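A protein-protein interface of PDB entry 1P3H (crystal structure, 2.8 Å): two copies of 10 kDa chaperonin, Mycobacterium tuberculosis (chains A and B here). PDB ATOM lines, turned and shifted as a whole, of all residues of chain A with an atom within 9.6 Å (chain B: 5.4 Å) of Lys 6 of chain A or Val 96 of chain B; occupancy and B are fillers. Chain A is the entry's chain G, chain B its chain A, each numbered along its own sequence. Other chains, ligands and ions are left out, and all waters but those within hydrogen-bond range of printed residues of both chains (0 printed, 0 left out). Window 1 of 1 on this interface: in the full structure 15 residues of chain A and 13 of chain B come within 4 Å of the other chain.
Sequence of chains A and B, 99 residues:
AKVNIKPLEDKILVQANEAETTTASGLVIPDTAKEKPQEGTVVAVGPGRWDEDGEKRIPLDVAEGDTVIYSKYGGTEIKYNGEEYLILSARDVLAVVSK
Printed residues of chain A that touch a printed residue of chain B: Lys 2, Val 3, Asn 4, Ile 5, Lys 6, Pro 7, Leu 8, Glu 9 and Lys 11. Hydrophobic or aromatic side chains of chain A within 4 Å of the printed part of chain B: Val 3, Ile 5 and Leu 8. Of the 11 printed residues of chain B, 7 touch a printed residue of chain A. Hydrophobic or aromatic side chains of chain B that line the printed part of chain A: Val 62, Ala 95, Val 96 and Val 97. Among the printed residues, no Asp or Glu carboxylate lies within 4 Å of a Lys or Arg side-chain nitrogen of the other chain.
Ser 98 of chain B touches Lys 2 of chain A. CG1 of Val 3 of chain A touches CG1 of Val 97 of chain B, at 3.4 Å. Val 3 of chain A touches Ser 98 of chain B (C to O, 3.98 Å). Val 96 of chain B touches Asn 4 of chain A (O to O, 3.8 Å). CA of Val 97 of chain B touches O of Asn 4 of chain A, at 3.6 Å. CG2 of Ile 5 of chain A touches CB of Ala 95 of chain B (3.7 Å). Ile 5 of chain A touches Val 96 of chain B (C to O, 3.7 Å). Lys 6 of chain A touches Ala 95 of chain B. Ala 95 of chain B touches Pro 7 of chain A. Leu 8 of chain A touches Asp 61 of chain B.
The backbone NH of Val 97 of chain B is in hydrogen-bond range of the backbone carbonyl oxygen of Thr 67 of chain B, at 2.7 Å. O of Ile 69 of chain B lies within hydrogen-bond range of N of Leu 94 of chain B, at 2.7 Å. O of Ala 95 of chain B lies within hydrogen-bond range of N of Ile 69 of chain B (2.9 Å). The backbone NH of Gly 46 of chain A sits at hydrogen-bond distance from the backbone carbonyl oxygen of Lys 11 of chain A (2.8 Å).
The backbone carbonyl oxygen (O) of Leu 94 of chain B is in hydrogen-bond range of the backbone NH (N) of Leu 8 of chain A (3.1 Å). The backbone NH (N) of Val 96 of chain B lies within hydrogen-bond range of the backbone carbonyl oxygen (O) of Lys 6 of chain A (2.6 Å). The backbone carbonyl oxygen of Asn 4 of chain A sits at hydrogen-bond distance from the backbone NH of Ser 98 of chain B, 2.9 Å away. OG of Ser 98 of chain B sits at hydrogen-bond distance from NZ of Lys 6 of chain A, at 3.0 Å. The side-chain carboxylate of Asp 61 of chain B sits close to the side-chain carboxylate of Glu 9 of chain A (2.9 Å).
Of chain B, only Ala 95 (2.9 Å), Val 96 (2.6 Å) and Ser 98 (3.0 Å) come within 4 Å of Lys 6 of chain A. Of chain A, only Asn 4, Ile 5, Lys 6 and Leu 8 come within 4 Å of Val 96 of chain B. Of chain A, only Ile 5, Lys 6 and Pro 7 come within 4 Å of Ala 95 of chain B. Val 97 of chain B touches just these residues of chain A: Val 3 and Asn 4. Of the printed residues of chain A, Val 62 of chain B touches Leu 8. Of the printed residues of chain B, Lys 11 of chain A touches Leu 94. Printed residues of chain B within 4 Å of Val 3 of chain A: Val 97 and Ser 98. Printed residues of chain B within 4 Å of Glu 9 of chain A: Asp 61 (2.9 Å). Of the printed residues of chain B, Asn 4 of chain A touches Val 96, Val 97 and Ser 98. Ala 44 of chain A touches none of the printed residues of chain B. Val 45 of chain A touches none of the printed residues of chain B. The nearest residue of chain B that does not touch Lys 6 of chain A is Leu 94 of chain B (4.6 Å). The nearest printed residue of chain A that does not touch Asp 61 of chain B is Pro 47 of chain A (4.9 Å).
No position is printed for both chains.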
ATOM      1  N   LYS A   2       0.841  18.404   0.941  1.00  0.00           N
ATOM      2  CA  LYS A   2      -0.484  17.868   0.619  1.00  0.00           C
ATOM      3  C   LYS A   2      -1.610  18.794   1.110  1.00  0.00           C
ATOM      4  O   LYS A   2      -1.472  19.480   2.137  1.00  0.00           O
ATOM      5  CB  LYS A   2      -0.669  16.481   1.255  1.00  0.00           C
ATOM      6  CG  LYS A   2      -1.249  15.470   0.306  1.00  0.00           C
ATOM      7  CD  LYS A   2      -0.121  14.697  -0.348  1.00  0.00           C
ATOM      8  CE  LYS A   2      -0.644  13.814  -1.472  1.00  0.00           C
ATOM      9  NZ  LYS A   2       0.474  13.070  -2.130  1.00  0.00           N
ATOM     10  N   VAL A   3      -2.717  18.804   0.363  1.00  0.00           N
ATOM     11  CA  VAL A   3      -3.867  19.629   0.711  1.00  0.00           C
ATOM     12  C   VAL A   3      -4.475  19.219   2.039  1.00  0.00           C
ATOM     13  O   VAL A   3      -4.829  18.070   2.252  1.00  0.00           O
ATOM     14  CB  VAL A   3      -4.946  19.570  -0.408  1.00  0.00           C
ATOM     15  CG1 VAL A   3      -6.203  20.326   0.002  1.00  0.00           C
ATOM     16  CG2 VAL A   3      -4.377  20.189  -1.695  1.00  0.00           C
ATOM     17  N   ASN A   4      -4.614  20.196   2.915  1.00  0.00           N
ATOM     18  CA  ASN A   4      -5.160  19.973   4.245  1.00  0.00           C
ATOM     19  C   ASN A   4      -6.341  20.941   4.499  1.00  0.00           C
ATOM     20  O   ASN A   4      -6.168  22.156   4.440  1.00  0.00           O
ATOM     21  CB  ASN A   4      -4.004  20.176   5.260  1.00  0.00           C
ATOM     22  CG  ASN A   4      -4.469  20.191   6.723  1.00  0.00           C
ATOM     23  OD1 ASN A   4      -5.049  19.223   7.225  1.00  0.00           O
ATOM     24  ND2 ASN A   4      -4.204  21.303   7.408  1.00  0.00           N
ATOM     25  N   ILE A   5      -7.538  20.399   4.745  1.00  0.00           N
ATOM     26  CA  ILE A   5      -8.723  21.216   5.023  1.00  0.00           C
ATOM     27  C   ILE A   5      -8.893  21.628   6.484  1.00  0.00           C
ATOM     28  O   ILE A   5      -9.014  20.785   7.356  1.00  0.00           O
ATOM     29  CB  ILE A   5     -10.006  20.491   4.583  1.00  0.00           C
ATOM     30  CG1 ILE A   5      -9.940  20.228   3.071  1.00  0.00           C
ATOM     31  CG2 ILE A   5     -11.238  21.303   4.992  1.00  0.00           C
ATOM     32  CD1 ILE A   5     -11.124  19.478   2.492  1.00  0.00           C
ATOM     33  N   LYS A   6      -8.929  22.938   6.725  1.00  0.00           N
ATOM     34  CA  LYS A   6      -9.069  23.491   8.068  1.00  0.00           C
ATOM     35  C   LYS A   6     -10.412  24.211   8.289  1.00  0.00           C
ATOM     36  O   LYS A   6     -10.653  25.283   7.746  1.00  0.00           O
ATOM     37  CB  LYS A   6      -7.910  24.458   8.327  1.00  0.00           C
ATOM     38  CG  LYS A   6      -6.555  23.850   8.028  1.00  0.00           C
ATOM     39  CD  LYS A   6      -5.463  24.899   7.914  1.00  0.00           C
ATOM     40  CE  LYS A   6      -4.115  24.299   8.311  1.00  0.00           C
ATOM     41  NZ  LYS A   6      -2.990  25.262   8.127  1.00  0.00           N
ATOM     42  N   PRO A   7     -11.302  23.618   9.086  1.00  0.00           N
ATOM     43  CA  PRO A   7     -12.640  24.114   9.428  1.00  0.00           C
ATOM     44  C   PRO A   7     -12.660  25.359  10.317  1.00  0.00           C
ATOM     45  O   PRO A   7     -12.022  25.375  11.358  1.00  0.00           O
ATOM     46  CB  PRO A   7     -13.286  22.920  10.116  1.00  0.00           C
ATOM     47  CG  PRO A   7     -12.591  21.761   9.477  1.00  0.00           C
ATOM     48  CD  PRO A   7     -11.169  22.208   9.477  1.00  0.00           C
ATOM     49  N   LEU A   8     -13.404  26.384   9.918  1.00  0.00           N
ATOM     50  CA  LEU A   8     -13.476  27.605  10.708  1.00  0.00           C
ATOM     51  C   LEU A   8     -14.551  27.424  11.741  1.00  0.00           C
ATOM     52  O   LEU A   8     -15.270  26.426  11.714  1.00  0.00           O
ATOM     53  CB  LEU A   8     -13.782  28.801   9.808  1.00  0.00           C
ATOM     54  CG  LEU A   8     -12.724  29.016   8.725  1.00  0.00           C
ATOM     55  CD1 LEU A   8     -13.221  30.039   7.753  1.00  0.00           C
ATOM     56  CD2 LEU A   8     -11.407  29.442   9.333  1.00  0.00           C
ATOM     57  N   GLU A   9     -14.654  28.384  12.653  1.00  0.00           N
ATOM     58  CA  GLU A   9     -15.646  28.330  13.725  1.00  0.00           C
ATOM     59  C   GLU A   9     -15.755  26.958  14.391  1.00  0.00           C
ATOM     60  O   GLU A   9     -14.746  26.300  14.642  1.00  0.00           O
ATOM     61  CB  GLU A   9     -17.024  28.767  13.198  1.00  0.00           C
ATOM     62  CG  GLU A   9     -17.411  30.186  13.639  1.00  0.00           C
ATOM     63  CD  GLU A   9     -16.599  31.287  12.948  1.00  0.00           C
ATOM     64  OE1 GLU A   9     -17.063  31.793  11.898  1.00  0.00           O
ATOM     65  OE2 GLU A   9     -15.501  31.639  13.455  1.00  0.00           O
ATOM     66  N   ASP A  10     -16.987  26.552  14.685  1.00  0.00           N
ATOM     67  CA  ASP A  10     -17.246  25.271  15.323  1.00  0.00           C
ATOM     68  C   ASP A  10     -17.625  24.202  14.301  1.00  0.00           C
ATOM     69  O   ASP A  10     -18.376  23.269  14.596  1.00  0.00           O
ATOM     70  CB  ASP A  10     -18.359  25.413  16.362  1.00  0.00           C
ATOM     71  CG  ASP A  10     -19.653  25.933  15.767  1.00  0.00           C
ATOM     72  OD1 ASP A  10     -20.680  25.929  16.483  1.00  0.00           O
ATOM     73  OD2 ASP A  10     -19.642  26.352  14.586  1.00  0.00           O
ATOM     74  N   LYS A  11     -17.110  24.338  13.089  1.00  0.00           N
ATOM     75  CA  LYS A  11     -17.405  23.354  12.061  1.00  0.00           C
ATOM     76  C   LYS A  11     -16.360  22.246  12.121  1.00  0.00           C
ATOM     77  O   LYS A  11     -15.259  22.450  12.614  1.00  0.00           O
ATOM     78  CB  LYS A  11     -17.381  24.015  10.681  1.00  0.00           C
ATOM     79  CG  LYS A  11     -18.248  25.256  10.589  1.00  0.00           C
ATOM     80  CD  LYS A  11     -18.180  25.887   9.217  1.00  0.00           C
ATOM     81  CE  LYS A  11     -18.793  27.270   9.234  1.00  0.00           C
ATOM     82  NZ  LYS A  11     -20.125  27.289   9.896  1.00  0.00           N
ATOM     83  N   ILE A  12     -16.706  21.063  11.636  1.00  0.00           N
ATOM     84  CA  ILE A  12     -15.751  19.983  11.635  1.00  0.00           C
ATOM     85  C   ILE A  12     -15.824  19.225  10.335  1.00  0.00           C
ATOM     86  O   ILE A  12     -16.841  19.214   9.668  1.00  0.00           O
ATOM     87  CB  ILE A  12     -16.009  18.992  12.747  1.00  0.00           C
ATOM     88  CG1 ILE A  12     -17.381  18.370  12.569  1.00  0.00           C
ATOM     89  CG2 ILE A  12     -15.921  19.687  14.084  1.00  0.00           C
ATOM     90  CD1 ILE A  12     -17.602  17.170  13.445  1.00  0.00           C
ATOM     91  N   LEU A  13     -14.716  18.598   9.975  1.00  0.00           N
ATOM     92  CA  LEU A  13     -14.656  17.812   8.765  1.00  0.00           C
ATOM     93  C   LEU A  13     -14.828  16.352   9.197  1.00  0.00           C
ATOM     94  O   LEU A  13     -14.131  15.862  10.084  1.00  0.00           O
ATOM     95  CB  LEU A  13     -13.308  18.010   8.080  1.00  0.00           C
ATOM     96  CG  LEU A  13     -13.252  17.388   6.697  1.00  0.00           C
ATOM     97  CD1 LEU A  13     -14.248  18.053   5.758  1.00  0.00           C
ATOM     98  CD2 LEU A  13     -11.865  17.541   6.181  1.00  0.00           C
ATOM     99  N   VAL A  43     -12.270  14.076  11.104  1.00  0.00           N
ATOM    100  CA  VAL A  43     -10.956  14.194  10.506  1.00  0.00           C
ATOM    101  C   VAL A  43     -10.263  15.485  10.878  1.00  0.00           C
ATOM    102  O   VAL A  43      -9.041  15.530  10.966  1.00  0.00           O
ATOM    103  CB  VAL A  43     -11.062  14.098   8.982  1.00  0.00           C
ATOM    104  CG1 VAL A  43      -9.688  14.119   8.354  1.00  0.00           C
ATOM    105  CG2 VAL A  43     -11.810  12.830   8.601  1.00  0.00           C
ATOM    106  N   ALA A  44     -11.042  16.535  11.081  1.00  0.00           N
ATOM    107  CA  ALA A  44     -10.488  17.828  11.443  1.00  0.00           C
ATOM    108  C   ALA A  44     -11.565  18.625  12.158  1.00  0.00           C
ATOM    109  O   ALA A  44     -12.751  18.476  11.868  1.00  0.00           O
ATOM    110  CB  ALA A  44     -10.031  18.554  10.212  1.00  0.00           C
ATOM    111  N   VAL A  45     -11.157  19.459  13.105  1.00  0.00           N
ATOM    112  CA  VAL A  45     -12.114  20.261  13.848  1.00  0.00           C
ATOM    113  C   VAL A  45     -11.747  21.734  13.809  1.00  0.00           C
ATOM    114  O   VAL A  45     -10.587  22.087  13.685  1.00  0.00           O
ATOM    115  CB  VAL A  45     -12.199  19.816  15.329  1.00  0.00           C
ATOM    116  CG1 VAL A  45     -12.573  18.344  15.404  1.00  0.00           C
ATOM    117  CG2 VAL A  45     -10.868  20.091  16.036  1.00  0.00           C
ATOM    118  N   GLY A  46     -12.754  22.592  13.908  1.00  0.00           N
ATOM    119  CA  GLY A  46     -12.498  24.016  13.917  1.00  0.00           C
ATOM    120  C   GLY A  46     -12.009  24.450  15.287  1.00  0.00           C
ATOM    121  O   GLY A  46     -12.071  23.674  16.252  1.00  0.00           O
ATOM    122  N   PRO A  47     -11.507  25.683  15.411  1.00  0.00           N
ATOM    123  CA  PRO A  47     -11.012  26.186  16.691  1.00  0.00           C
ATOM    124  C   PRO A  47     -12.137  26.289  17.701  1.00  0.00           C
ATOM    125  O   PRO A  47     -11.915  26.147  18.903  1.00  0.00           O
ATOM    126  CB  PRO A  47     -10.449  27.541  16.327  1.00  0.00           C
ATOM    127  CG  PRO A  47     -11.369  27.990  15.243  1.00  0.00           C
ATOM    128  CD  PRO A  47     -11.473  26.742  14.391  1.00  0.00           C
ATOM    129  N   ILE A  87     -18.536  18.716   5.746  1.00  0.00           N
ATOM    130  CA  ILE A  87     -18.205  19.818   6.630  1.00  0.00           C
ATOM    131  C   ILE A  87     -19.519  20.215   7.276  1.00  0.00           C
ATOM    132  O   ILE A  87     -20.458  20.606   6.590  1.00  0.00           O
ATOM    133  CB  ILE A  87     -17.647  21.039   5.877  1.00  0.00           C
ATOM    134  CG1 ILE A  87     -16.409  20.651   5.078  1.00  0.00           C
ATOM    135  CG2 ILE A  87     -17.269  22.128   6.868  1.00  0.00           C
ATOM    136  CD1 ILE A  87     -15.862  21.777   4.238  1.00  0.00           C
ATOM    137  N   ASP B  61     -11.565  34.829  10.857  1.00  0.00           N
ATOM    138  CA  ASP B  61     -10.624  33.721  10.871  1.00  0.00           C
ATOM    139  C   ASP B  61     -10.005  33.454   9.523  1.00  0.00           C
ATOM    140  O   ASP B  61      -9.485  32.372   9.280  1.00  0.00           O
ATOM    141  CB  ASP B  61     -11.292  32.459  11.394  1.00  0.00           C
ATOM    142  CG  ASP B  61     -11.583  32.541  12.868  1.00  0.00           C
ATOM    143  OD1 ASP B  61     -10.665  32.876  13.632  1.00  0.00           O
ATOM    144  OD2 ASP B  61     -12.728  32.278  13.268  1.00  0.00           O
ATOM    145  N   VAL B  62     -10.076  34.439   8.640  1.00  0.00           N
ATOM    146  CA  VAL B  62      -9.486  34.301   7.318  1.00  0.00           C
ATOM    147  C   VAL B  62      -8.643  35.526   7.064  1.00  0.00           C
ATOM    148  O   VAL B  62      -8.850  36.571   7.680  1.00  0.00           O
ATOM    149  CB  VAL B  62     -10.551  34.155   6.200  1.00  0.00           C
ATOM    150  CG1 VAL B  62     -11.294  32.852   6.372  1.00  0.00           C
ATOM    151  CG2 VAL B  62     -11.506  35.323   6.228  1.00  0.00           C
ATOM    152  N   ASP B  66      -5.501  33.423   1.884  1.00  0.00           N
ATOM    153  CA  ASP B  66      -6.070  32.158   2.304  1.00  0.00           C
ATOM    154  C   ASP B  66      -6.944  31.598   1.217  1.00  0.00           C
ATOM    155  O   ASP B  66      -7.678  32.324   0.558  1.00  0.00           O
ATOM    156  CB  ASP B  66      -6.919  32.322   3.559  1.00  0.00           C
ATOM    157  CG  ASP B  66      -6.086  32.558   4.804  1.00  0.00           C
ATOM    158  OD1 ASP B  66      -4.858  32.378   4.720  1.00  0.00           O
ATOM    159  OD2 ASP B  66      -6.649  32.904   5.865  1.00  0.00           O
ATOM    160  N   THR B  67      -6.843  30.293   1.018  1.00  0.00           N
ATOM    161  CA  THR B  67      -7.672  29.628   0.044  1.00  0.00           C
ATOM    162  C   THR B  67      -8.760  29.091   0.923  1.00  0.00           C
ATOM    163  O   THR B  67      -8.509  28.501   1.967  1.00  0.00           O
ATOM    164  CB  THR B  67      -6.929  28.515  -0.635  1.00  0.00           C
ATOM    165  OG1 THR B  67      -5.817  29.071  -1.345  1.00  0.00           O
ATOM    166  CG2 THR B  67      -7.852  27.780  -1.603  1.00  0.00           C
ATOM    167  N   VAL B  68      -9.980  29.314   0.504  1.00  0.00           N
ATOM    168  CA  VAL B  68     -11.073  28.902   1.321  1.00  0.00           C
ATOM    169  C   VAL B  68     -12.123  28.188   0.540  1.00  0.00           C
ATOM    170  O   VAL B  68     -12.096  28.182  -0.685  1.00  0.00           O
ATOM    171  CB  VAL B  68     -11.689  30.122   1.930  1.00  0.00           C
ATOM    172  CG1 VAL B  68     -10.753  30.691   2.964  1.00  0.00           C
ATOM    173  CG2 VAL B  68     -11.947  31.158   0.808  1.00  0.00           C
ATOM    174  N   ILE B  69     -13.042  27.575   1.275  1.00  0.00           N
ATOM    175  CA  ILE B  69     -14.178  26.879   0.707  1.00  0.00           C
ATOM    176  C   ILE B  69     -15.362  27.676   1.247  1.00  0.00           C
ATOM    177  O   ILE B  69     -15.434  27.982   2.445  1.00  0.00           O
ATOM    178  CB  ILE B  69     -14.259  25.419   1.179  1.00  0.00           C
ATOM    179  CG1 ILE B  69     -13.082  24.638   0.585  1.00  0.00           C
ATOM    180  CG2 ILE B  69     -15.597  24.792   0.767  1.00  0.00           C
ATOM    181  CD1 ILE B  69     -12.940  23.252   1.143  1.00  0.00           C
ATOM    182  N   LEU B  94     -16.561  28.139   4.936  1.00  0.00           N
ATOM    183  CA  LEU B  94     -16.611  26.857   5.609  1.00  0.00           C
ATOM    184  C   LEU B  94     -15.283  26.437   6.215  1.00  0.00           C
ATOM    185  O   LEU B  94     -15.219  26.080   7.384  1.00  0.00           O
ATOM    186  CB  LEU B  94     -17.107  25.803   4.634  1.00  0.00           C
ATOM    187  CG  LEU B  94     -18.472  26.156   4.052  1.00  0.00           C
ATOM    188  CD1 LEU B  94     -18.807  25.234   2.904  1.00  0.00           C
ATOM    189  CD2 LEU B  94     -19.519  26.065   5.127  1.00  0.00           C
ATOM    190  N   ALA B  95     -14.218  26.493   5.428  1.00  0.00           N
ATOM    191  CA  ALA B  95     -12.915  26.083   5.917  1.00  0.00           C
ATOM    192  C   ALA B  95     -11.818  26.686   5.076  1.00  0.00           C
ATOM    193  O   ALA B  95     -12.057  27.147   3.970  1.00  0.00           O
ATOM    194  CB  ALA B  95     -12.809  24.580   5.882  1.00  0.00           C
ATOM    195  N   VAL B  96     -10.609  26.685   5.611  1.00  0.00           N
ATOM    196  CA  VAL B  96      -9.471  27.211   4.890  1.00  0.00           C
ATOM    197  C   VAL B  96      -8.715  26.004   4.392  1.00  0.00           C
ATOM    198  O   VAL B  96      -8.553  25.034   5.119  1.00  0.00           O
ATOM    199  CB  VAL B  96      -8.544  28.012   5.795  1.00  0.00           C
ATOM    200  CG1 VAL B  96      -7.413  28.591   4.976  1.00  0.00           C
ATOM    201  CG2 VAL B  96      -9.309  29.116   6.480  1.00  0.00           C
ATOM    202  N   VAL B  97      -8.257  26.057   3.150  1.00  0.00           N
ATOM    203  CA  VAL B  97      -7.520  24.948   2.558  1.00  0.00           C
ATOM    204  C   VAL B  97      -6.048  25.314   2.468  1.00  0.00           C
ATOM    205  O   VAL B  97      -5.697  26.341   1.893  1.00  0.00           O
ATOM    206  CB  VAL B  97      -8.035  24.638   1.142  1.00  0.00           C
ATOM    207  CG1 VAL B  97      -7.290  23.464   0.558  1.00  0.00           C
ATOM    208  CG2 VAL B  97      -9.502  24.334   1.197  1.00  0.00           C
ATOM    209  N   SER B  98      -5.170  24.458   2.978  1.00  0.00           N
ATOM    210  CA  SER B  98      -3.728  24.741   2.936  1.00  0.00           C
ATOM    211  C   SER B  98      -2.833  23.537   2.637  1.00  0.00           C
ATOM    212  O   SER B  98      -2.810  22.572   3.395  1.00  0.00           O
ATOM    213  CB  SER B  98      -3.297  25.384   4.258  1.00  0.00           C
ATOM    214  OG  SER B  98      -3.905  24.726   5.355  1.00  0.00           O
